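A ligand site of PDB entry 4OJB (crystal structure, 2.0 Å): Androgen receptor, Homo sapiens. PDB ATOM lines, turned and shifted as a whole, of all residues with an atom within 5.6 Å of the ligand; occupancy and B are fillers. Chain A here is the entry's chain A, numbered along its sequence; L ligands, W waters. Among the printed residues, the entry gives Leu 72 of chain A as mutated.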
ATOM      1  N   LEU A  32      18.215   1.727  36.505  1.00  0.00           N
ATOM      2  CA  LEU A  32      17.025   1.087  35.984  1.00  0.00           C
ATOM      3  C   LEU A  32      15.836   2.027  35.874  1.00  0.00           C
ATOM      4  O   LEU A  32      15.080   1.913  34.924  1.00  0.00           O
ATOM      5  CB  LEU A  32      16.656  -0.153  36.786  1.00  0.00           C
ATOM      6  CG  LEU A  32      17.188  -1.476  36.220  1.00  0.00           C
ATOM      7  CD1 LEU A  32      16.611  -1.714  34.829  1.00  0.00           C
ATOM      8  CD2 LEU A  32      18.713  -1.530  36.166  1.00  0.00           C
ATOM      9  N   LEU A  35      16.625   3.677  32.690  1.00  0.00           N
ATOM     10  CA  LEU A  35      16.303   2.782  31.554  1.00  0.00           C
ATOM     11  C   LEU A  35      14.802   2.698  31.267  1.00  0.00           C
ATOM     12  O   LEU A  35      14.440   2.652  30.121  1.00  0.00           O
ATOM     13  CB  LEU A  35      16.910   1.399  31.742  1.00  0.00           C
ATOM     14  CG  LEU A  35      18.385   1.239  31.360  1.00  0.00           C
ATOM     15  CD1 LEU A  35      18.939  -0.131  31.764  1.00  0.00           C
ATOM     16  CD2 LEU A  35      18.543   1.416  29.856  1.00  0.00           C
ATOM     17  N   ASN A  36      13.952   2.670  32.315  1.00  0.00           N
ATOM     18  CA  ASN A  36      12.508   2.585  32.187  1.00  0.00           C
ATOM     19  C   ASN A  36      11.953   3.888  31.621  1.00  0.00           C
ATOM     20  O   ASN A  36      11.107   3.873  30.745  1.00  0.00           O
ATOM     21  CB  ASN A  36      11.828   2.392  33.545  1.00  0.00           C
ATOM     22  CG  ASN A  36      12.170   1.067  34.207  1.00  0.00           C
ATOM     23  OD1 ASN A  36      12.581   0.101  33.553  1.00  0.00           O
ATOM     24  ND2 ASN A  36      11.897   0.991  35.542  1.00  0.00           N
ATOM     25  N   GLU A  37      12.527   4.985  32.041  1.00  0.00           N
ATOM     26  CA  GLU A  37      12.114   6.271  31.504  1.00  0.00           C
ATOM     27  C   GLU A  37      12.551   6.387  30.041  1.00  0.00           C
ATOM     28  O   GLU A  37      11.804   6.857  29.183  1.00  0.00           O
ATOM     29  CB  GLU A  37      12.657   7.432  32.336  1.00  0.00           C
ATOM     30  CG  GLU A  37      12.401   8.807  31.706  1.00  0.00           C
ATOM     31  CD  GLU A  37      10.917   9.209  31.666  1.00  0.00           C
ATOM     32  OE1 GLU A  37      10.541  10.056  30.833  1.00  0.00           O
ATOM     33  OE2 GLU A  37      10.119   8.724  32.481  1.00  0.00           O
ATOM     34  N   LEU A  38      13.744   5.947  29.746  1.00  0.00           N
ATOM     35  CA  LEU A  38      14.209   5.912  28.385  1.00  0.00           C
ATOM     36  C   LEU A  38      13.337   5.036  27.510  1.00  0.00           C
ATOM     37  O   LEU A  38      13.023   5.416  26.380  1.00  0.00           O
ATOM     38  CB  LEU A  38      15.683   5.470  28.316  1.00  0.00           C
ATOM     39  CG  LEU A  38      16.241   5.460  26.899  1.00  0.00           C
ATOM     40  CD1 LEU A  38      16.181   6.855  26.272  1.00  0.00           C
ATOM     41  CD2 LEU A  38      17.637   4.892  26.885  1.00  0.00           C
ATOM     42  N   GLY A  39      12.897   3.894  28.026  1.00  0.00           N
ATOM     43  CA  GLY A  39      12.039   2.992  27.237  1.00  0.00           C
ATOM     44  C   GLY A  39      10.724   3.715  26.843  1.00  0.00           C
ATOM     45  O   GLY A  39      10.293   3.633  25.706  1.00  0.00           O
ATOM     46  N   GLU A  40      10.124   4.444  27.777  1.00  0.00           N
ATOM     47  CA  GLU A  40       8.937   5.243  27.470  1.00  0.00           C
ATOM     48  C   GLU A  40       9.159   6.319  26.420  1.00  0.00           C
ATOM     49  O   GLU A  40       8.318   6.543  25.601  1.00  0.00           O
ATOM     50  CB  GLU A  40       8.398   5.953  28.712  1.00  0.00           C
ATOM     51  CG  GLU A  40       7.143   6.747  28.339  1.00  0.00           C
ATOM     52  CD  GLU A  40       6.222   6.910  29.506  1.00  0.00           C
ATOM     53  OE1 GLU A  40       5.354   6.032  29.711  1.00  0.00           O
ATOM     54  OE2 GLU A  40       6.447   7.902  30.247  1.00  0.00           O
ATOM     55  N   GLN A  42      11.483   6.286  24.146  1.00  0.00           N
ATOM     56  CA  GLN A  42      11.695   5.662  22.843  1.00  0.00           C
ATOM     57  C   GLN A  42      10.381   5.080  22.264  1.00  0.00           C
ATOM     58  O   GLN A  42      10.170   5.174  21.060  1.00  0.00           O
ATOM     59  CB  GLN A  42      12.828   4.594  22.869  1.00  0.00           C
ATOM     60  CG  GLN A  42      14.234   5.167  23.120  1.00  0.00           C
ATOM     61  CD  GLN A  42      15.371   4.158  22.903  1.00  0.00           C
ATOM     62  OE1 GLN A  42      16.559   4.393  23.256  1.00  0.00           O
ATOM     63  NE2 GLN A  42      15.036   3.049  22.276  1.00  0.00           N
ATOM     64  N   GLN A  69       3.878  -2.809  20.293  1.00  0.00           N
ATOM     65  CA  GLN A  69       4.193  -3.200  21.649  1.00  0.00           C
ATOM     66  C   GLN A  69       4.997  -4.522  21.741  1.00  0.00           C
ATOM     67  O   GLN A  69       5.984  -4.592  22.502  1.00  0.00           O
ATOM     68  CB  GLN A  69       2.924  -3.246  22.461  1.00  0.00           C
ATOM     69  CG  GLN A  69       2.445  -1.857  22.747  1.00  0.00           C
ATOM     70  CD  GLN A  69       1.057  -1.801  23.322  1.00  0.00           C
ATOM     71  OE1 GLN A  69       0.369  -2.786  23.404  1.00  0.00           O
ATOM     72  NE2 GLN A  69       0.621  -0.587  23.629  1.00  0.00           N
ATOM     73  N   LEU A  72       8.642  -3.808  20.381  1.00  0.00           N
ATOM     74  CA  LEU A  72       9.380  -2.698  20.927  1.00  0.00           C
ATOM     75  C   LEU A  72      10.751  -3.086  21.451  1.00  0.00           C
ATOM     76  O   LEU A  72      11.742  -2.438  21.131  1.00  0.00           O
ATOM     77  CB  LEU A  72       8.579  -1.987  22.065  1.00  0.00           C
ATOM     78  CG  LEU A  72       9.313  -0.835  22.704  1.00  0.00           C
ATOM     79  CD1 LEU A  72       9.520   0.372  21.730  1.00  0.00           C
ATOM     80  CD2 LEU A  72       8.621  -0.388  24.005  1.00  0.00           C
ATOM     81  N   MET A  73      10.808  -4.089  22.315  1.00  0.00           N
ATOM     82  CA  MET A  73      12.127  -4.516  22.882  1.00  0.00           C
ATOM     83  C   MET A  73      13.166  -4.838  21.803  1.00  0.00           C
ATOM     84  O   MET A  73      14.260  -4.275  21.825  1.00  0.00           O
ATOM     85  CB  MET A  73      11.966  -5.688  23.843  1.00  0.00           C
ATOM     86  CG  MET A  73      13.209  -5.967  24.691  1.00  0.00           C
ATOM     87  SD  MET A  73      13.634  -4.653  25.805  1.00  0.00           S
ATOM     88  CE  MET A  73      12.478  -5.089  27.103  1.00  0.00           C
ATOM     89  N   MET A  76      14.321  -1.741  19.944  1.00  0.00           N
ATOM     90  CA  MET A  76      15.195  -0.878  20.732  1.00  0.00           C
ATOM     91  C   MET A  76      16.617  -1.498  20.804  1.00  0.00           C
ATOM     92  O   MET A  76      17.647  -0.800  20.747  1.00  0.00           O
ATOM     93  CB  MET A  76      14.641  -0.675  22.161  1.00  0.00           C
ATOM     94  CG  MET A  76      13.332   0.203  22.258  1.00  0.00           C
ATOM     95  SD  MET A  76      13.022   0.709  23.970  1.00  0.00           S
ATOM     96  CE  MET A  76      12.944  -0.840  24.829  1.00  0.00           C
ATOM     97  N   VAL A  77      16.642  -2.822  20.907  1.00  0.00           N
ATOM     98  CA  VAL A  77      17.874  -3.545  21.015  1.00  0.00           C
ATOM     99  C   VAL A  77      18.661  -3.386  19.762  1.00  0.00           C
ATOM    100  O   VAL A  77      19.839  -3.073  19.826  1.00  0.00           O
ATOM    101  CB  VAL A  77      17.636  -5.028  21.274  1.00  0.00           C
ATOM    102  CG1 VAL A  77      18.894  -5.830  20.931  1.00  0.00           C
ATOM    103  CG2 VAL A  77      17.221  -5.188  22.714  1.00  0.00           C
ATOM    104  N   MET A  80      19.900   0.110  19.297  1.00  0.00           N
ATOM    105  CA  MET A  80      20.937   0.471  20.235  1.00  0.00           C
ATOM    106  C   MET A  80      22.278  -0.219  19.818  1.00  0.00           C
ATOM    107  O   MET A  80      23.357   0.350  19.968  1.00  0.00           O
ATOM    108  CB  MET A  80      20.517   0.126  21.623  1.00  0.00           C
ATOM    109  CG  MET A  80      21.447   0.539  22.738  1.00  0.00           C
ATOM    110  SD  MET A  80      22.850  -0.567  23.024  1.00  0.00           S
ATOM    111  CE  MET A  80      22.011  -2.039  23.714  1.00  0.00           C
ATOM    112  N   ARG A  83      23.640   2.134  17.211  1.00  0.00           N
ATOM    113  CA  ARG A  83      24.192   3.371  17.840  1.00  0.00           C
ATOM    114  C   ARG A  83      25.556   3.108  18.486  1.00  0.00           C
ATOM    115  O   ARG A  83      26.487   3.896  18.336  1.00  0.00           O
ATOM    116  CB  ARG A  83      23.231   3.963  18.927  1.00  0.00           C
ATOM    117  CG  ARG A  83      22.064   4.728  18.371  1.00  0.00           C
ATOM    118  CD  ARG A  83      21.379   5.580  19.447  1.00  0.00           C
ATOM    119  NE  ARG A  83      20.912   4.791  20.571  1.00  0.00           N
ATOM    120  CZ  ARG A  83      19.829   4.042  20.566  1.00  0.00           C
ATOM    121  NH1 ARG A  83      19.046   3.964  19.508  1.00  0.00           N
ATOM    122  NH2 ARG A  83      19.508   3.390  21.678  1.00  0.00           N
ATOM    123  N   TYR A  94      25.636   2.207  24.001  1.00  0.00           N
ATOM    124  CA  TYR A  94      25.119   3.549  23.873  1.00  0.00           C
ATOM    125  C   TYR A  94      23.559   3.611  23.918  1.00  0.00           C
ATOM    126  O   TYR A  94      22.880   3.837  22.901  1.00  0.00           O
ATOM    127  CB  TYR A  94      25.653   4.078  22.602  1.00  0.00           C
ATOM    128  CG  TYR A  94      25.766   5.544  22.475  1.00  0.00           C
ATOM    129  CD1 TYR A  94      24.679   6.296  21.979  1.00  0.00           C
ATOM    130  CD2 TYR A  94      26.956   6.211  22.742  1.00  0.00           C
ATOM    131  CE1 TYR A  94      24.748   7.661  21.809  1.00  0.00           C
ATOM    132  CE2 TYR A  94      27.045   7.607  22.582  1.00  0.00           C
ATOM    133  CZ  TYR A  94      25.924   8.313  22.104  1.00  0.00           C
ATOM    134  OH  TYR A  94      25.935   9.677  21.907  1.00  0.00           O
ATOM    135  N   PHE A  95      23.012   3.454  25.103  1.00  0.00           N
ATOM    136  CA  PHE A  95      21.567   3.448  25.206  1.00  0.00           C
ATOM    137  C   PHE A  95      21.021   4.829  24.802  1.00  0.00           C
ATOM    138  O   PHE A  95      20.034   4.937  24.094  1.00  0.00           O
ATOM    139  CB  PHE A  95      21.136   3.137  26.589  1.00  0.00           C
ATOM    140  CG  PHE A  95      21.376   1.705  27.000  1.00  0.00           C
ATOM    141  CD1 PHE A  95      20.445   0.732  26.705  1.00  0.00           C
ATOM    142  CD2 PHE A  95      22.472   1.344  27.698  1.00  0.00           C
ATOM    143  CE1 PHE A  95      20.656  -0.581  27.107  1.00  0.00           C
ATOM    144  CE2 PHE A  95      22.688   0.018  28.082  1.00  0.00           C
ATOM    145  CZ  PHE A  95      21.760  -0.938  27.810  1.00  0.00           C
ATOM    146  N   MET A 111      22.188  -6.772  34.536  1.00  0.00           N
ATOM    147  CA  MET A 111      21.806  -7.183  33.206  1.00  0.00           C
ATOM    148  C   MET A 111      23.057  -7.522  32.458  1.00  0.00           C
ATOM    149  O   MET A 111      23.138  -7.313  31.230  1.00  0.00           O
ATOM    150  CB  MET A 111      21.111  -6.019  32.462  1.00  0.00           C
ATOM    151  CG  MET A 111      20.047  -5.280  33.207  1.00  0.00           C
ATOM    152  SD  MET A 111      19.379  -3.923  32.184  1.00  0.00           S
ATOM    153  CE  MET A 111      18.499  -4.928  31.009  1.00  0.00           C
ATOM    154  N   MET A 118      24.251  -7.994  23.709  1.00  0.00           N
ATOM    155  CA  MET A 118      23.951  -6.786  22.890  1.00  0.00           C
ATOM    156  C   MET A 118      25.221  -6.225  22.367  1.00  0.00           C
ATOM    157  O   MET A 118      25.277  -5.745  21.220  1.00  0.00           O
ATOM    158  CB  MET A 118      23.165  -5.741  23.687  1.00  0.00           C
ATOM    159  CG  MET A 118      21.744  -6.169  23.962  1.00  0.00           C
ATOM    160  SD  MET A 118      20.723  -4.987  24.868  1.00  0.00           S
ATOM    161  CE  MET A 118      21.302  -4.929  26.524  1.00  0.00           C
ATOM    162  N   LEU A 204      15.450  -9.919  27.940  1.00  0.00           N
ATOM    163  CA  LEU A 204      15.175  -8.604  28.530  1.00  0.00           C
ATOM    164  C   LEU A 204      13.770  -8.538  29.030  1.00  0.00           C
ATOM    165  O   LEU A 204      13.454  -7.891  30.008  1.00  0.00           O
ATOM    166  CB  LEU A 204      15.480  -7.500  27.511  1.00  0.00           C
ATOM    167  CG  LEU A 204      16.973  -7.250  27.290  1.00  0.00           C
ATOM    168  CD1 LEU A 204      17.220  -6.338  26.135  1.00  0.00           C
ATOM    169  CD2 LEU A 204      17.666  -6.732  28.554  1.00  0.00           C
ATOM    170  N   HIS A 205      12.864  -9.101  28.243  1.00  0.00           N
ATOM    171  CA  HIS A 205      11.505  -9.215  28.671  1.00  0.00           C
ATOM    172  C   HIS A 205      11.344  -9.948  29.950  1.00  0.00           C
ATOM    173  O   HIS A 205      10.538  -9.510  30.811  1.00  0.00           O
ATOM    174  CB  HIS A 205      10.658  -9.955  27.662  1.00  0.00           C
ATOM    175  CG  HIS A 205      10.205  -9.112  26.537  1.00  0.00           C
ATOM    176  ND1 HIS A 205      10.235  -9.552  25.242  1.00  0.00           N
ATOM    177  CD2 HIS A 205       9.756  -7.828  26.511  1.00  0.00           C
ATOM    178  CE1 HIS A 205       9.746  -8.600  24.454  1.00  0.00           C
ATOM    179  NE2 HIS A 205       9.434  -7.563  25.201  1.00  0.00           N
ATOM    180  N   PHE A 207      13.609 -10.273  32.319  1.00  0.00           N
ATOM    181  CA  PHE A 207      14.217  -9.411  33.379  1.00  0.00           C
ATOM    182  C   PHE A 207      13.296  -8.277  33.783  1.00  0.00           C
ATOM    183  O   PHE A 207      13.063  -7.997  34.984  1.00  0.00           O
ATOM    184  CB  PHE A 207      15.589  -8.908  32.909  1.00  0.00           C
ATOM    185  CG  PHE A 207      16.149  -7.778  33.735  1.00  0.00           C
ATOM    186  CD1 PHE A 207      15.815  -6.464  33.454  1.00  0.00           C
ATOM    187  CD2 PHE A 207      17.083  -8.021  34.763  1.00  0.00           C
ATOM    188  CE1 PHE A 207      16.343  -5.400  34.217  1.00  0.00           C
ATOM    189  CE2 PHE A 207      17.622  -6.983  35.526  1.00  0.00           C
ATOM    190  CZ  PHE A 207      17.246  -5.664  35.264  1.00  0.00           C
ATOM    191  N   THR A 208      12.698  -7.658  32.775  1.00  0.00           N
ATOM    192  CA  THR A 208      11.751  -6.555  32.995  1.00  0.00           C
ATOM    193  C   THR A 208      10.494  -6.915  33.714  1.00  0.00           C
ATOM    194  O   THR A 208       9.989  -6.137  34.556  1.00  0.00           O
ATOM    195  CB  THR A 208      11.313  -5.901  31.627  1.00  0.00           C
ATOM    196  OG1 THR A 208      12.494  -5.336  31.009  1.00  0.00           O
ATOM    197  CG2 THR A 208      10.272  -4.859  31.834  1.00  0.00           C
ATOM    198  N   LEU A 211      11.361  -7.546  37.340  1.00  0.00           N
ATOM    199  CA  LEU A 211      11.639  -6.285  37.998  1.00  0.00           C
ATOM    200  C   LEU A 211      10.391  -5.501  38.318  1.00  0.00           C
ATOM    201  O   LEU A 211      10.302  -4.829  39.345  1.00  0.00           O
ATOM    202  CB  LEU A 211      12.572  -5.452  37.103  1.00  0.00           C
ATOM    203  CG  LEU A 211      13.168  -4.188  37.706  1.00  0.00           C
ATOM    204  CD1 LEU A 211      14.029  -4.609  38.889  1.00  0.00           C
ATOM    205  CD2 LEU A 211      14.002  -3.462  36.665  1.00  0.00           C
ATOM    206  N   PHE A 222       8.571   2.650  37.483  1.00  0.00           N
ATOM    207  CA  PHE A 222       8.085   2.450  36.089  1.00  0.00           C
ATOM    208  C   PHE A 222       7.140   3.496  35.696  1.00  0.00           C
ATOM    209  O   PHE A 222       6.214   3.756  36.430  1.00  0.00           O
ATOM    210  CB  PHE A 222       7.390   1.123  35.882  1.00  0.00           C
ATOM    211  CG  PHE A 222       8.330  -0.003  35.905  1.00  0.00           C
ATOM    212  CD1 PHE A 222       8.766  -0.510  37.117  1.00  0.00           C
ATOM    213  CD2 PHE A 222       8.866  -0.487  34.737  1.00  0.00           C
ATOM    214  CE1 PHE A 222       9.723  -1.522  37.179  1.00  0.00           C
ATOM    215  CE2 PHE A 222       9.777  -1.518  34.785  1.00  0.00           C
ATOM    216  CZ  PHE A 222      10.197  -2.039  36.009  1.00  0.00           C
ATOM    217  N   MET A 226       4.584   2.011  30.560  1.00  0.00           N
ATOM    218  CA  MET A 226       5.514   0.898  30.479  1.00  0.00           C
ATOM    219  C   MET A 226       5.048  -0.201  31.412  1.00  0.00           C
ATOM    220  O   MET A 226       5.103  -1.351  31.006  1.00  0.00           O
ATOM    221  CB  MET A 226       6.922   1.311  30.782  1.00  0.00           C
ATOM    222  CG  MET A 226       7.414   2.436  29.871  1.00  0.00           C
ATOM    223  SD  MET A 226       6.921   2.300  28.118  1.00  0.00           S
ATOM    224  CE  MET A 226       8.279   1.163  27.788  1.00  0.00           C
ATOM    225  N   ILE A 229       2.124  -1.953  29.621  1.00  0.00           N
ATOM    226  CA  ILE A 229       2.653  -2.879  28.627  1.00  0.00           C
ATOM    227  C   ILE A 229       3.299  -4.108  29.258  1.00  0.00           C
ATOM    228  O   ILE A 229       3.108  -5.205  28.787  1.00  0.00           O
ATOM    229  CB  ILE A 229       3.669  -2.193  27.624  1.00  0.00           C
ATOM    230  CG1 ILE A 229       2.945  -1.236  26.655  1.00  0.00           C
ATOM    231  CG2 ILE A 229       4.471  -3.170  26.803  1.00  0.00           C
ATOM    232  CD1 ILE A 229       3.830  -0.115  26.102  1.00  0.00           C
ATOM    233  N   ILE A 230       4.089  -3.928  30.304  1.00  0.00           N
ATOM    234  CA  ILE A 230       4.765  -5.021  30.888  1.00  0.00           C
ATOM    235  C   ILE A 230       3.778  -6.018  31.531  1.00  0.00           C
ATOM    236  O   ILE A 230       4.084  -7.209  31.599  1.00  0.00           O
ATOM    237  CB  ILE A 230       5.789  -4.575  31.958  1.00  0.00           C
ATOM    238  CG1 ILE A 230       6.913  -3.736  31.338  1.00  0.00           C
ATOM    239  CG2 ILE A 230       6.408  -5.808  32.631  1.00  0.00           C
ATOM    240  CD1 ILE A 230       7.626  -2.867  32.335  1.00  0.00           C
ATOM    241  N   VAL A 234       3.673  -8.146  27.711  1.00  0.00           N
ATOM    242  CA  VAL A 234       4.909  -8.951  27.859  1.00  0.00           C
ATOM    243  C   VAL A 234       4.606 -10.411  28.364  1.00  0.00           C
ATOM    244  O   VAL A 234       5.229 -11.339  27.898  1.00  0.00           O
ATOM    245  CB  VAL A 234       5.920  -8.233  28.775  1.00  0.00           C
ATOM    246  CG1 VAL A 234       7.089  -9.131  29.129  1.00  0.00           C
ATOM    247  CG2 VAL A 234       6.476  -6.954  28.069  1.00  0.00           C
HETATM  248  C1  LIG L   1      10.895  -2.179  27.154  1.00  0.00           C
HETATM  249  C2  LIG L   1      10.177  -2.952  26.255  1.00  0.00           C
HETATM  250  C3  LIG L   1       8.945  -3.441  26.609  1.00  0.00           C
HETATM  251  F1  LIG L   1       8.161  -4.213  25.822  1.00  0.00           F
HETATM  252  C4  LIG L   1       8.402  -3.129  27.811  1.00  0.00           C
HETATM  253  C5  LIG L   1       9.097  -2.366  28.712  1.00  0.00           C
HETATM  254  C6  LIG L   1      10.341  -1.858  28.403  1.00  0.00           C
HETATM  255  S1  LIG L   1      11.112  -0.959  29.520  1.00  0.00           S
HETATM  256  O1  LIG L   1      11.970  -0.082  28.743  1.00  0.00           O
HETATM  257  O2  LIG L   1      10.201  -0.321  30.472  1.00  0.00           O
HETATM  258  C7  LIG L   1      12.094  -1.962  30.460  1.00  0.00           C
HETATM  259  C8  LIG L   1      13.545  -1.506  30.640  1.00  0.00           C
HETATM  260  O3  LIG L   1      13.625  -0.237  31.318  1.00  0.00           O
HETATM  261  C9  LIG L   1      14.281  -2.473  31.579  1.00  0.00           C
HETATM  262  C10 LIG L   1      14.289  -1.486  29.307  1.00  0.00           C
HETATM  263  O4  LIG L   1      14.456  -2.516  28.653  1.00  0.00           O
HETATM  264  N1  LIG L   1      14.722  -0.273  28.907  1.00  0.00           N
HETATM  265  C11 LIG L   1      15.500  -0.067  27.804  1.00  0.00           C
HETATM  266  C12 LIG L   1      16.122  -1.074  27.055  1.00  0.00           C
HETATM  267  C13 LIG L   1      15.581   1.262  27.344  1.00  0.00           C
HETATM  268  C14 LIG L   1      16.313   1.610  26.226  1.00  0.00           C
HETATM  269  C15 LIG L   1      16.905   0.660  25.449  1.00  0.00           C
HETATM  270  C16 LIG L   1      17.564   1.121  24.461  1.00  0.00           C
HETATM  271  N2  LIG L   1      18.191   1.513  23.578  1.00  0.00           N
HETATM  272  C17 LIG L   1      16.849  -0.750  25.902  1.00  0.00           C
HETATM  273  C18 LIG L   1      17.495  -1.814  25.059  1.00  0.00           C
HETATM  274  F2  LIG L   1      16.653  -2.381  24.275  1.00  0.00           F
HETATM  275  F3  LIG L   1      18.405  -1.352  24.246  1.00  0.00           F
HETATM  276  F4  LIG L   1      17.934  -2.718  25.855  1.00  0.00           F
HETATM  277  O   HOH W   1      17.055   2.096  20.657  1.00  0.00           O
HETATM  278  O   HOH W   2       8.439  -5.531  23.337  1.00  0.00           O
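An oxygen (O3) of the ligand sits at hydrogen-bond distance from the backbone NH (N) of Asn 36.
An oxygen (O3) of the ligand lies within hydrogen-bond range of the side-chain amide oxygen of Asn 36 (2.5 Å).
NH2 of Arg 83 lies within hydrogen-bond range of N2 of the ligand (3.0 Å).
O of Leu 35 lies within hydrogen-bond range of N1 of the ligand (3.2 Å).
A nitrogen (N2) of the ligand sits close to the side-chain amide oxygen of Gln 42, 3.3 Å away.
The side-chain amide nitrogen of Asn 36 sits close to the backbone carbonyl oxygen of Leu 32, 3.4 Å away.
The guanidinium group (NH2) of Arg 83 sits at hydrogen-bond distance from the side-chain amide oxygen (OE1) of Gln 42, at 3.5 Å.
O of Phe 95 lies within hydrogen-bond range of NH2 of Arg 83, at 2.9 Å.
The backbone carbonyl oxygen (O) of Tyr 94 sits at hydrogen-bond distance from the guanidinium group (NE) of Arg 83, at 3.2 Å.
SD of Met 76 sits close to NE2 of Gln 42.
The side-chain hydroxyl (OG1) of Thr 208 is in hydrogen-bond range of the backbone carbonyl oxygen (O) of Leu 204 (2.9 Å).
The backbone carbonyl oxygen (O) of Ile 229 is in hydrogen-bond range of the backbone NH (N) of Val 234 (3.2 Å).
The side-chain sulfur (SD) of Met 73 sits close to an oxygen (O4) of the ligand (3.7 Å).
F2 of the ligand sits close to N of Val 77 (3.4 Å).
SD of Met 118 lies close to F4 of the ligand (3.7 Å).
Leu 38 touches the ligand (CD2 to C14, 3.6 Å).
CA of Gly 39 touches O1 of the ligand, 3.4 Å away.
Gln 69 touches the ligand (O to F1, 3.99 Å).
CD2 of Leu 72 touches C2 of the ligand, at 3.7 Å.
CE of Met 76 touches C1 of the ligand (3.4 Å).
Met 80 touches the ligand (CB to N2, 3.3 Å).
Phe 95 touches the ligand.
CD1 of Leu 204 touches F4 of the ligand, 3.7 Å away.
His 205 touches the ligand (NE2 to F1, 3.6 Å).
Thr 208 touches the ligand (OG1 to C9, 3.4 Å).
Met 226 touches the ligand.
Ile 229 touches the ligand (CG2 to F1, 3.96 Å).
Ile 230 touches the ligand (CG1 to C5, 3.7 Å).
Val 234 touches the ligand.
21 residues have an atom within 4 Å of the ligand: Leu 35, Asn 36, Leu 38, Gly 39, Gln 42, Gln 69, Leu 72, Met 73, Met 76, Val 77, Met 80, Arg 83, Phe 95, Met 118, Leu 204, His 205, Thr 208, Met 226, Ile 229, Ile 230 and Val 234.
The nearest printed residue that does not touch the ligand is Leu 32 (4.1 Å).
Water W2 lies within hydrogen-bond range of the backbone carbonyl oxygen (O) of Gln 69 (2.8 Å), a ring nitrogen (NE2) of His 205 (2.9 Å), the backbone NH (N) of Met 73 (3.0 Å) and the backbone NH (N) of Leu 72 (3.4 Å).
Water W1 lies within hydrogen-bond range of NE2 of Gln 42, NH2 of Arg 83, O of Met 76 and N2 of the ligand.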
